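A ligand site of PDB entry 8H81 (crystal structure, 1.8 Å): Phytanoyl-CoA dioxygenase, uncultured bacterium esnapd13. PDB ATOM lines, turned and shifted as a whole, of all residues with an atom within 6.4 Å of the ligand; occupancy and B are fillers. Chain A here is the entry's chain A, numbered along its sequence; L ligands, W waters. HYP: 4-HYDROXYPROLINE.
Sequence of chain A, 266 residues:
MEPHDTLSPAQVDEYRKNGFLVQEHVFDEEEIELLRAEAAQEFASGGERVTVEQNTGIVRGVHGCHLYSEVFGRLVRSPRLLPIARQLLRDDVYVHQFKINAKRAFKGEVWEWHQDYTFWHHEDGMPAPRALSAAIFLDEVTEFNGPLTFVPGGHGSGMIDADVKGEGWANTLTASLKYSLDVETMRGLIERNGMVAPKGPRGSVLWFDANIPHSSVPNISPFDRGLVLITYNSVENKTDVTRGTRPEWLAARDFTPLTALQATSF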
ATOM      1  N   HIS A  63     -27.110 -25.039 -16.326  1.00  0.00           N
ATOM      2  CA  HIS A  63     -26.384 -25.971 -17.177  1.00  0.00           C
ATOM      3  C   HIS A  63     -25.738 -27.083 -16.350  1.00  0.00           C
ATOM      4  O   HIS A  63     -25.233 -26.847 -15.251  1.00  0.00           O
ATOM      5  CB  HIS A  63     -25.338 -25.201 -17.994  1.00  0.00           C
ATOM      6  CG  HIS A  63     -25.908 -24.124 -18.859  1.00  0.00           C
ATOM      7  ND1 HIS A  63     -26.323 -22.909 -18.387  1.00  0.00           N
ATOM      8  CD2 HIS A  63     -26.126 -24.135 -20.206  1.00  0.00           C
ATOM      9  CE1 HIS A  63     -26.802 -22.191 -19.403  1.00  0.00           C
ATOM     10  NE2 HIS A  63     -26.682 -22.925 -20.541  1.00  0.00           N
ATOM     11  N   HIS A  96     -23.795 -34.903 -23.863  1.00  0.00           N
ATOM     12  CA  HIS A  96     -22.810 -33.862 -24.111  1.00  0.00           C
ATOM     13  C   HIS A  96     -23.106 -32.638 -23.248  1.00  0.00           C
ATOM     14  O   HIS A  96     -22.193 -32.038 -22.665  1.00  0.00           O
ATOM     15  CB  HIS A  96     -22.798 -33.468 -25.588  1.00  0.00           C
ATOM     16  CG  HIS A  96     -21.922 -32.300 -25.899  1.00  0.00           C
ATOM     17  ND1 HIS A  96     -20.557 -32.310 -25.695  1.00  0.00           N
ATOM     18  CD2 HIS A  96     -22.247 -31.065 -26.366  1.00  0.00           C
ATOM     19  CE1 HIS A  96     -20.067 -31.120 -26.030  1.00  0.00           C
ATOM     20  NE2 HIS A  96     -21.090 -30.335 -26.452  1.00  0.00           N
ATOM     21  N   GLN A  97     -24.384 -32.247 -23.220  1.00  0.00           N
ATOM     22  CA  GLN A  97     -24.821 -31.006 -22.608  1.00  0.00           C
ATOM     23  C   GLN A  97     -26.232 -31.184 -22.062  1.00  0.00           C
ATOM     24  O   GLN A  97     -27.045 -31.913 -22.641  1.00  0.00           O
ATOM     25  CB  GLN A  97     -24.736 -29.870 -23.630  1.00  0.00           C
ATOM     26  CG  GLN A  97     -25.166 -28.507 -23.105  1.00  0.00           C
ATOM     27  CD  GLN A  97     -24.875 -27.413 -24.107  1.00  0.00           C
ATOM     28  OE1 GLN A  97     -25.724 -27.047 -24.909  1.00  0.00           O
ATOM     29  NE2 GLN A  97     -23.640 -26.922 -24.097  1.00  0.00           N
ATOM     30  N   LYS A  99     -29.219 -28.520 -20.226  1.00  0.00           N
ATOM     31  CA  LYS A  99     -29.553 -27.159 -19.846  1.00  0.00           C
ATOM     32  C   LYS A  99     -31.059 -27.030 -19.677  1.00  0.00           C
ATOM     33  O   LYS A  99     -31.845 -27.745 -20.297  1.00  0.00           O
ATOM     34  CB  LYS A  99     -28.980 -26.163 -20.859  1.00  0.00           C
ATOM     35  CG  LYS A  99     -29.428 -26.320 -22.302  1.00  0.00           C
ATOM     36  CD  LYS A  99     -28.714 -25.381 -23.268  1.00  0.00           C
ATOM     37  CE  LYS A  99     -29.053 -25.650 -24.722  1.00  0.00           C
ATOM     38  NZ  LYS A  99     -28.532 -26.958 -25.184  1.00  0.00           N
ATOM     39  N   ASN A 101     -33.881 -24.022 -19.969  1.00  0.00           N
ATOM     40  CA  ASN A 101     -34.138 -22.692 -20.501  1.00  0.00           C
ATOM     41  C   ASN A 101     -35.584 -22.304 -20.183  1.00  0.00           C
ATOM     42  O   ASN A 101     -36.502 -22.898 -20.742  1.00  0.00           O
ATOM     43  CB  ASN A 101     -33.911 -22.615 -22.019  1.00  0.00           C
ATOM     44  CG  ASN A 101     -32.463 -22.717 -22.463  1.00  0.00           C
ATOM     45  OD1 ASN A 101     -31.533 -22.620 -21.656  1.00  0.00           O
ATOM     46  ND2 ASN A 101     -32.264 -22.887 -23.760  1.00  0.00           N
ATOM     47  N   TRP A 111     -34.042 -14.944 -29.583  1.00  0.00           N
ATOM     48  CA  TRP A 111     -32.874 -15.803 -29.713  1.00  0.00           C
ATOM     49  C   TRP A 111     -32.450 -15.887 -31.179  1.00  0.00           C
ATOM     50  O   TRP A 111     -33.193 -16.409 -32.007  1.00  0.00           O
ATOM     51  CB  TRP A 111     -33.142 -17.211 -29.172  1.00  0.00           C
ATOM     52  CG  TRP A 111     -33.090 -17.298 -27.678  1.00  0.00           C
ATOM     53  CD1 TRP A 111     -33.964 -16.735 -26.783  1.00  0.00           C
ATOM     54  CD2 TRP A 111     -32.096 -17.983 -26.904  1.00  0.00           C
ATOM     55  NE1 TRP A 111     -33.582 -17.025 -25.499  1.00  0.00           N
ATOM     56  CE2 TRP A 111     -32.438 -17.793 -25.541  1.00  0.00           C
ATOM     57  CE3 TRP A 111     -30.954 -18.738 -27.214  1.00  0.00           C
ATOM     58  CZ2 TRP A 111     -31.674 -18.344 -24.504  1.00  0.00           C
ATOM     59  CZ3 TRP A 111     -30.209 -19.278 -26.188  1.00  0.00           C
ATOM     60  CH2 TRP A 111     -30.559 -19.077 -24.856  1.00  0.00           C
ATOM     61  N   HIS A 114     -29.414 -19.854 -35.193  1.00  0.00           N
ATOM     62  CA  HIS A 114     -28.169 -20.558 -35.005  1.00  0.00           C
ATOM     63  C   HIS A 114     -28.349 -22.065 -35.182  1.00  0.00           C
ATOM     64  O   HIS A 114     -29.473 -22.576 -35.184  1.00  0.00           O
ATOM     65  CB  HIS A 114     -27.584 -20.276 -33.611  1.00  0.00           C
ATOM     66  CG  HIS A 114     -28.424 -20.790 -32.473  1.00  0.00           C
ATOM     67  ND1 HIS A 114     -29.681 -20.313 -32.173  1.00  0.00           N
ATOM     68  CD2 HIS A 114     -28.139 -21.770 -31.567  1.00  0.00           C
ATOM     69  CE1 HIS A 114     -30.149 -20.969 -31.112  1.00  0.00           C
ATOM     70  NE2 HIS A 114     -29.216 -21.887 -30.728  1.00  0.00           N
ATOM     71  N   GLN A 115     -27.202 -22.747 -35.346  1.00  0.00           N
ATOM     72  CA  GLN A 115     -27.100 -24.198 -35.288  1.00  0.00           C
ATOM     73  C   GLN A 115     -26.272 -24.563 -34.060  1.00  0.00           C
ATOM     74  O   GLN A 115     -25.194 -24.008 -33.860  1.00  0.00           O
ATOM     75  CB  GLN A 115     -26.423 -24.739 -36.553  1.00  0.00           C
ATOM     76  CG  GLN A 115     -27.179 -24.465 -37.845  1.00  0.00           C
ATOM     77  CD  GLN A 115     -26.342 -24.762 -39.063  1.00  0.00           C
ATOM     78  OE1 GLN A 115     -25.319 -24.125 -39.307  1.00  0.00           O
ATOM     79  NE2 GLN A 115     -26.772 -25.730 -39.852  1.00  0.00           N
ATOM     80  N   ASP A 116     -26.765 -25.509 -33.254  1.00  0.00           N
ATOM     81  CA  ASP A 116     -26.075 -25.955 -32.049  1.00  0.00           C
ATOM     82  C   ASP A 116     -24.700 -26.537 -32.386  1.00  0.00           C
ATOM     83  O   ASP A 116     -23.734 -26.307 -31.652  1.00  0.00           O
ATOM     84  CB  ASP A 116     -26.867 -27.035 -31.298  1.00  0.00           C
ATOM     85  CG  ASP A 116     -28.090 -26.530 -30.553  1.00  0.00           C
ATOM     86  OD1 ASP A 116     -28.163 -25.313 -30.297  1.00  0.00           O
ATOM     87  OD2 ASP A 116     -28.981 -27.361 -30.251  1.00  0.00           O
ATOM     88  N   TYR A 117     -24.625 -27.303 -33.479  1.00  0.00           N
ATOM     89  CA  TYR A 117     -23.402 -28.036 -33.801  1.00  0.00           C
ATOM     90  C   TYR A 117     -22.216 -27.083 -33.999  1.00  0.00           C
ATOM     91  O   TYR A 117     -21.085 -27.444 -33.697  1.00  0.00           O
ATOM     92  CB  TYR A 117     -23.595 -28.910 -35.039  1.00  0.00           C
ATOM     93  CG  TYR A 117     -22.324 -29.573 -35.504  1.00  0.00           C
ATOM     94  CD1 TYR A 117     -21.634 -30.451 -34.679  1.00  0.00           C
ATOM     95  CD2 TYR A 117     -21.775 -29.288 -36.752  1.00  0.00           C
ATOM     96  CE1 TYR A 117     -20.447 -31.046 -35.098  1.00  0.00           C
ATOM     97  CE2 TYR A 117     -20.598 -29.872 -37.172  1.00  0.00           C
ATOM     98  CZ  TYR A 117     -19.929 -30.761 -36.350  1.00  0.00           C
ATOM     99  OH  TYR A 117     -18.756 -31.349 -36.756  1.00  0.00           O
ATOM    100  N   PHE A 119     -21.409 -24.512 -32.336  1.00  0.00           N
ATOM    101  CA  PHE A 119     -20.828 -24.268 -31.024  1.00  0.00           C
ATOM    102  C   PHE A 119     -20.022 -25.492 -30.585  1.00  0.00           C
ATOM    103  O   PHE A 119     -18.888 -25.380 -30.145  1.00  0.00           O
ATOM    104  CB  PHE A 119     -21.900 -23.967 -29.985  1.00  0.00           C
ATOM    105  CG  PHE A 119     -22.663 -22.689 -30.208  1.00  0.00           C
ATOM    106  CD1 PHE A 119     -23.648 -22.598 -31.189  1.00  0.00           C
ATOM    107  CD2 PHE A 119     -22.396 -21.564 -29.446  1.00  0.00           C
ATOM    108  CE1 PHE A 119     -24.345 -21.423 -31.397  1.00  0.00           C
ATOM    109  CE2 PHE A 119     -23.100 -20.386 -29.647  1.00  0.00           C
ATOM    110  CZ  PHE A 119     -24.064 -20.315 -30.627  1.00  0.00           C
ATOM    111  N   TRP A 120     -20.632 -26.676 -30.715  1.00  0.00           N
ATOM    112  CA  TRP A 120     -20.043 -27.904 -30.203  1.00  0.00           C
ATOM    113  C   TRP A 120     -18.793 -28.254 -30.994  1.00  0.00           C
ATOM    114  O   TRP A 120     -17.807 -28.726 -30.432  1.00  0.00           O
ATOM    115  CB  TRP A 120     -21.092 -29.021 -30.199  1.00  0.00           C
ATOM    116  CG  TRP A 120     -22.279 -28.706 -29.350  1.00  0.00           C
ATOM    117  CD1 TRP A 120     -22.329 -27.835 -28.295  1.00  0.00           C
ATOM    118  CD2 TRP A 120     -23.615 -29.207 -29.506  1.00  0.00           C
ATOM    119  NE1 TRP A 120     -23.598 -27.780 -27.781  1.00  0.00           N
ATOM    120  CE2 TRP A 120     -24.401 -28.609 -28.509  1.00  0.00           C
ATOM    121  CE3 TRP A 120     -24.212 -30.107 -30.392  1.00  0.00           C
ATOM    122  CZ2 TRP A 120     -25.761 -28.886 -28.353  1.00  0.00           C
ATOM    123  CZ3 TRP A 120     -25.559 -30.383 -30.255  1.00  0.00           C
ATOM    124  CH2 TRP A 120     -26.319 -29.769 -29.253  1.00  0.00           C
ATOM    125  N   GLU A 123     -16.198 -24.971 -30.176  1.00  0.00           N
ATOM    126  CA  GLU A 123     -15.882 -24.758 -28.769  1.00  0.00           C
ATOM    127  C   GLU A 123     -15.427 -26.051 -28.090  1.00  0.00           C
ATOM    128  O   GLU A 123     -14.576 -26.000 -27.206  1.00  0.00           O
ATOM    129  CB  GLU A 123     -17.097 -24.213 -28.003  1.00  0.00           C
ATOM    130  CG  GLU A 123     -17.616 -22.886 -28.516  1.00  0.00           C
ATOM    131  CD  GLU A 123     -16.651 -21.723 -28.365  1.00  0.00           C
ATOM    132  OE1 GLU A 123     -16.182 -21.491 -27.226  1.00  0.00           O
ATOM    133  OE2 GLU A 123     -16.370 -21.053 -29.377  1.00  0.00           O
ATOM    134  N   ASP A 124     -16.009 -27.191 -28.483  1.00  0.00           N
ATOM    135  CA  ASP A 124     -15.880 -28.415 -27.701  1.00  0.00           C
ATOM    136  C   ASP A 124     -15.118 -29.517 -28.457  1.00  0.00           C
ATOM    137  O   ASP A 124     -14.755 -30.525 -27.850  1.00  0.00           O
ATOM    138  CB  ASP A 124     -17.239 -28.937 -27.244  1.00  0.00           C
ATOM    139  CG  ASP A 124     -18.097 -27.916 -26.529  1.00  0.00           C
ATOM    140  OD1 ASP A 124     -17.528 -27.099 -25.760  1.00  0.00           O
ATOM    141  OD2 ASP A 124     -19.323 -27.945 -26.713  1.00  0.00           O
ATOM    142  N   TRP A 169     -16.180 -18.018 -24.144  1.00  0.00           N
ATOM    143  CA  TRP A 169     -17.443 -18.738 -24.330  1.00  0.00           C
ATOM    144  C   TRP A 169     -18.598 -18.063 -23.575  1.00  0.00           C
ATOM    145  O   TRP A 169     -19.701 -18.611 -23.550  1.00  0.00           O
ATOM    146  CB  TRP A 169     -17.280 -20.209 -23.917  1.00  0.00           C
ATOM    147  CG  TRP A 169     -16.715 -20.440 -22.546  1.00  0.00           C
ATOM    148  CD1 TRP A 169     -15.417 -20.763 -22.246  1.00  0.00           C
ATOM    149  CD2 TRP A 169     -17.422 -20.443 -21.285  1.00  0.00           C
ATOM    150  NE1 TRP A 169     -15.258 -20.923 -20.899  1.00  0.00           N
ATOM    151  CE2 TRP A 169     -16.469 -20.744 -20.283  1.00  0.00           C
ATOM    152  CE3 TRP A 169     -18.741 -20.195 -20.910  1.00  0.00           C
ATOM    153  CZ2 TRP A 169     -16.816 -20.801 -18.931  1.00  0.00           C
ATOM    154  CZ3 TRP A 169     -19.081 -20.264 -19.575  1.00  0.00           C
ATOM    155  CH2 TRP A 169     -18.132 -20.562 -18.596  1.00  0.00           C
ATOM    156  N   THR A 172     -21.844 -17.764 -25.533  1.00  0.00           N
ATOM    157  CA  THR A 172     -22.440 -18.976 -26.084  1.00  0.00           C
ATOM    158  C   THR A 172     -23.802 -19.260 -25.443  1.00  0.00           C
ATOM    159  O   THR A 172     -24.549 -20.081 -25.949  1.00  0.00           O
ATOM    160  CB  THR A 172     -21.494 -20.175 -25.931  1.00  0.00           C
ATOM    161  OG1 THR A 172     -21.191 -20.358 -24.550  1.00  0.00           O
ATOM    162  CG2 THR A 172     -20.209 -20.028 -26.722  1.00  0.00           C
ATOM    163  N   LEU A 173     -24.090 -18.596 -24.321  1.00  0.00           N
ATOM    164  CA  LEU A 173     -25.293 -18.862 -23.536  1.00  0.00           C
ATOM    165  C   LEU A 173     -26.218 -17.652 -23.493  1.00  0.00           C
ATOM    166  O   LEU A 173     -27.248 -17.690 -22.832  1.00  0.00           O
ATOM    167  CB  LEU A 173     -24.865 -19.248 -22.117  1.00  0.00           C
ATOM    168  CG  LEU A 173     -23.786 -20.325 -21.999  1.00  0.00           C
ATOM    169  CD1 LEU A 173     -23.472 -20.613 -20.537  1.00  0.00           C
ATOM    170  CD2 LEU A 173     -24.228 -21.602 -22.710  1.00  0.00           C
ATOM    171  N   LEU A 177     -25.649 -14.281 -29.388  1.00  0.00           N
ATOM    172  CA  LEU A 177     -24.936 -15.539 -29.539  1.00  0.00           C
ATOM    173  C   LEU A 177     -23.632 -15.330 -30.291  1.00  0.00           C
ATOM    174  O   LEU A 177     -23.534 -14.474 -31.172  1.00  0.00           O
ATOM    175  CB  LEU A 177     -25.828 -16.548 -30.279  1.00  0.00           C
ATOM    176  CG  LEU A 177     -26.897 -17.239 -29.432  1.00  0.00           C
ATOM    177  CD1 LEU A 177     -27.690 -18.214 -30.283  1.00  0.00           C
ATOM    178  CD2 LEU A 177     -26.272 -17.961 -28.244  1.00  0.00           C
ATOM    179  N   HIS A 214     -32.222 -22.811 -35.665  1.00  0.00           N
ATOM    180  CA  HIS A 214     -33.381 -22.478 -34.840  1.00  0.00           C
ATOM    181  C   HIS A 214     -33.228 -21.132 -34.160  1.00  0.00           C
ATOM    182  O   HIS A 214     -32.124 -20.612 -33.993  1.00  0.00           O
ATOM    183  CB  HIS A 214     -33.670 -23.598 -33.821  1.00  0.00           C
ATOM    184  CG  HIS A 214     -32.603 -23.876 -32.812  1.00  0.00           C
ATOM    185  ND1 HIS A 214     -31.467 -24.594 -33.098  1.00  0.00           N
ATOM    186  CD2 HIS A 214     -32.559 -23.599 -31.479  1.00  0.00           C
ATOM    187  CE1 HIS A 214     -30.737 -24.713 -31.995  1.00  0.00           C
ATOM    188  NE2 HIS A 214     -31.395 -24.106 -30.967  1.00  0.00           N
ATOM    189  N   ARG A 246     -14.268 -25.518 -22.715  1.00  0.00           N
ATOM    190  CA  ARG A 246     -15.329 -25.151 -21.777  1.00  0.00           C
ATOM    191  C   ARG A 246     -15.398 -26.153 -20.626  1.00  0.00           C
ATOM    192  O   ARG A 246     -14.879 -27.264 -20.739  1.00  0.00           O
ATOM    193  CB  ARG A 246     -16.659 -25.035 -22.527  1.00  0.00           C
ATOM    194  CG  ARG A 246     -16.621 -24.076 -23.708  1.00  0.00           C
ATOM    195  CD  ARG A 246     -17.995 -23.635 -24.155  1.00  0.00           C
ATOM    196  NE  ARG A 246     -18.787 -24.716 -24.712  1.00  0.00           N
ATOM    197  CZ  ARG A 246     -20.015 -24.583 -25.206  1.00  0.00           C
ATOM    198  NH1 ARG A 246     -20.640 -23.420 -25.113  1.00  0.00           N
ATOM    199  NH2 ARG A 246     -20.609 -25.615 -25.782  1.00  0.00           N
ATOM    200  N   LEU A 250     -20.703 -27.622 -19.295  1.00  0.00           N
ATOM    201  CA  LEU A 250     -21.145 -27.215 -20.627  1.00  0.00           C
ATOM    202  C   LEU A 250     -20.842 -28.291 -21.670  1.00  0.00           C
ATOM    203  O   LEU A 250     -21.585 -28.440 -22.638  1.00  0.00           O
ATOM    204  CB  LEU A 250     -20.467 -25.899 -21.017  1.00  0.00           C
ATOM    205  CG  LEU A 250     -20.996 -24.637 -20.345  1.00  0.00           C
ATOM    206  CD1 LEU A 250     -20.326 -23.400 -20.915  1.00  0.00           C
ATOM    207  CD2 LEU A 250     -22.511 -24.534 -20.465  1.00  0.00           C
HETATM  208  N   HYP L   1     -25.829 -22.590 -26.578  1.00  0.00           N
HETATM  209  CA  HYP L   1     -25.349 -23.971 -26.682  1.00  0.00           C
HETATM  210  C   HYP L   1     -23.821 -24.037 -26.470  1.00  0.00           C
HETATM  211  O   HYP L   1     -23.295 -25.139 -26.384  1.00  0.00           O
HETATM  212  CB  HYP L   1     -25.750 -24.411 -28.105  1.00  0.00           C
HETATM  213  CG  HYP L   1     -26.860 -23.440 -28.496  1.00  0.00           C
HETATM  214  CD  HYP L   1     -26.437 -22.155 -27.843  1.00  0.00           C
HETATM  215  OD1 HYP L   1     -28.103 -23.893 -27.987  1.00  0.00           O
HETATM  216  OXT HYP L   1     -23.250 -22.965 -26.393  1.00  0.00           O
HETATM  217  O   HOH W   1     -27.886 -22.326 -24.777  1.00  0.00           O
HETATM  218  O   HOH W   2     -30.466 -22.600 -25.978  1.00  0.00           O
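OD2 of Asp 124 lies within salt-bridge range of NH2 of Arg 246 (2.8 Å).
The backbone carbonyl oxygen (O) of Trp 169 lies within hydrogen-bond range of the side-chain hydroxyl (OG1) of Thr 172.
NE2 of Gln 97 is in hydrogen-bond range of O of Leu 250.
The guanidinium group of Arg 246 lies within hydrogen-bond range of the side-chain hydroxyl of Thr 172 (3.2 Å).
N of His 214 is in hydrogen-bond range of O of His 114 (2.8 Å).
The side-chain amino group (NZ) of Lys 99 is in hydrogen-bond range of the side-chain amide oxygen (OE1) of Gln 97, 2.8 Å away.
OD1 of Asp 116 is in hydrogen-bond range of OD1 of the ligand, 2.7 Å away.
NE1 of Trp 120 lies within hydrogen-bond range of O of the ligand (3.0 Å).
N of the ligand sits at hydrogen-bond distance from O of Thr 172.
NH2 of Arg 246 lies within salt-bridge range of O of the ligand (2.8 Å).
The side-chain amide nitrogen (NE2) of Gln 97 sits at hydrogen-bond distance from an oxygen (O) of the ligand (2.9 Å).
Water W2 lies within hydrogen-bond range of ND2 of Asn 101 (2.9 Å) and OD1 of the ligand (3.4 Å).
Merely in contact with the ligand: Lys 99, His 114 and Phe 119.
Hydrophobic or aromatic side chains that line the ligand: His 114, Phe 119 and Trp 120.
Of the 21 residues printed, 8 come within 4 Å of the ligand.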
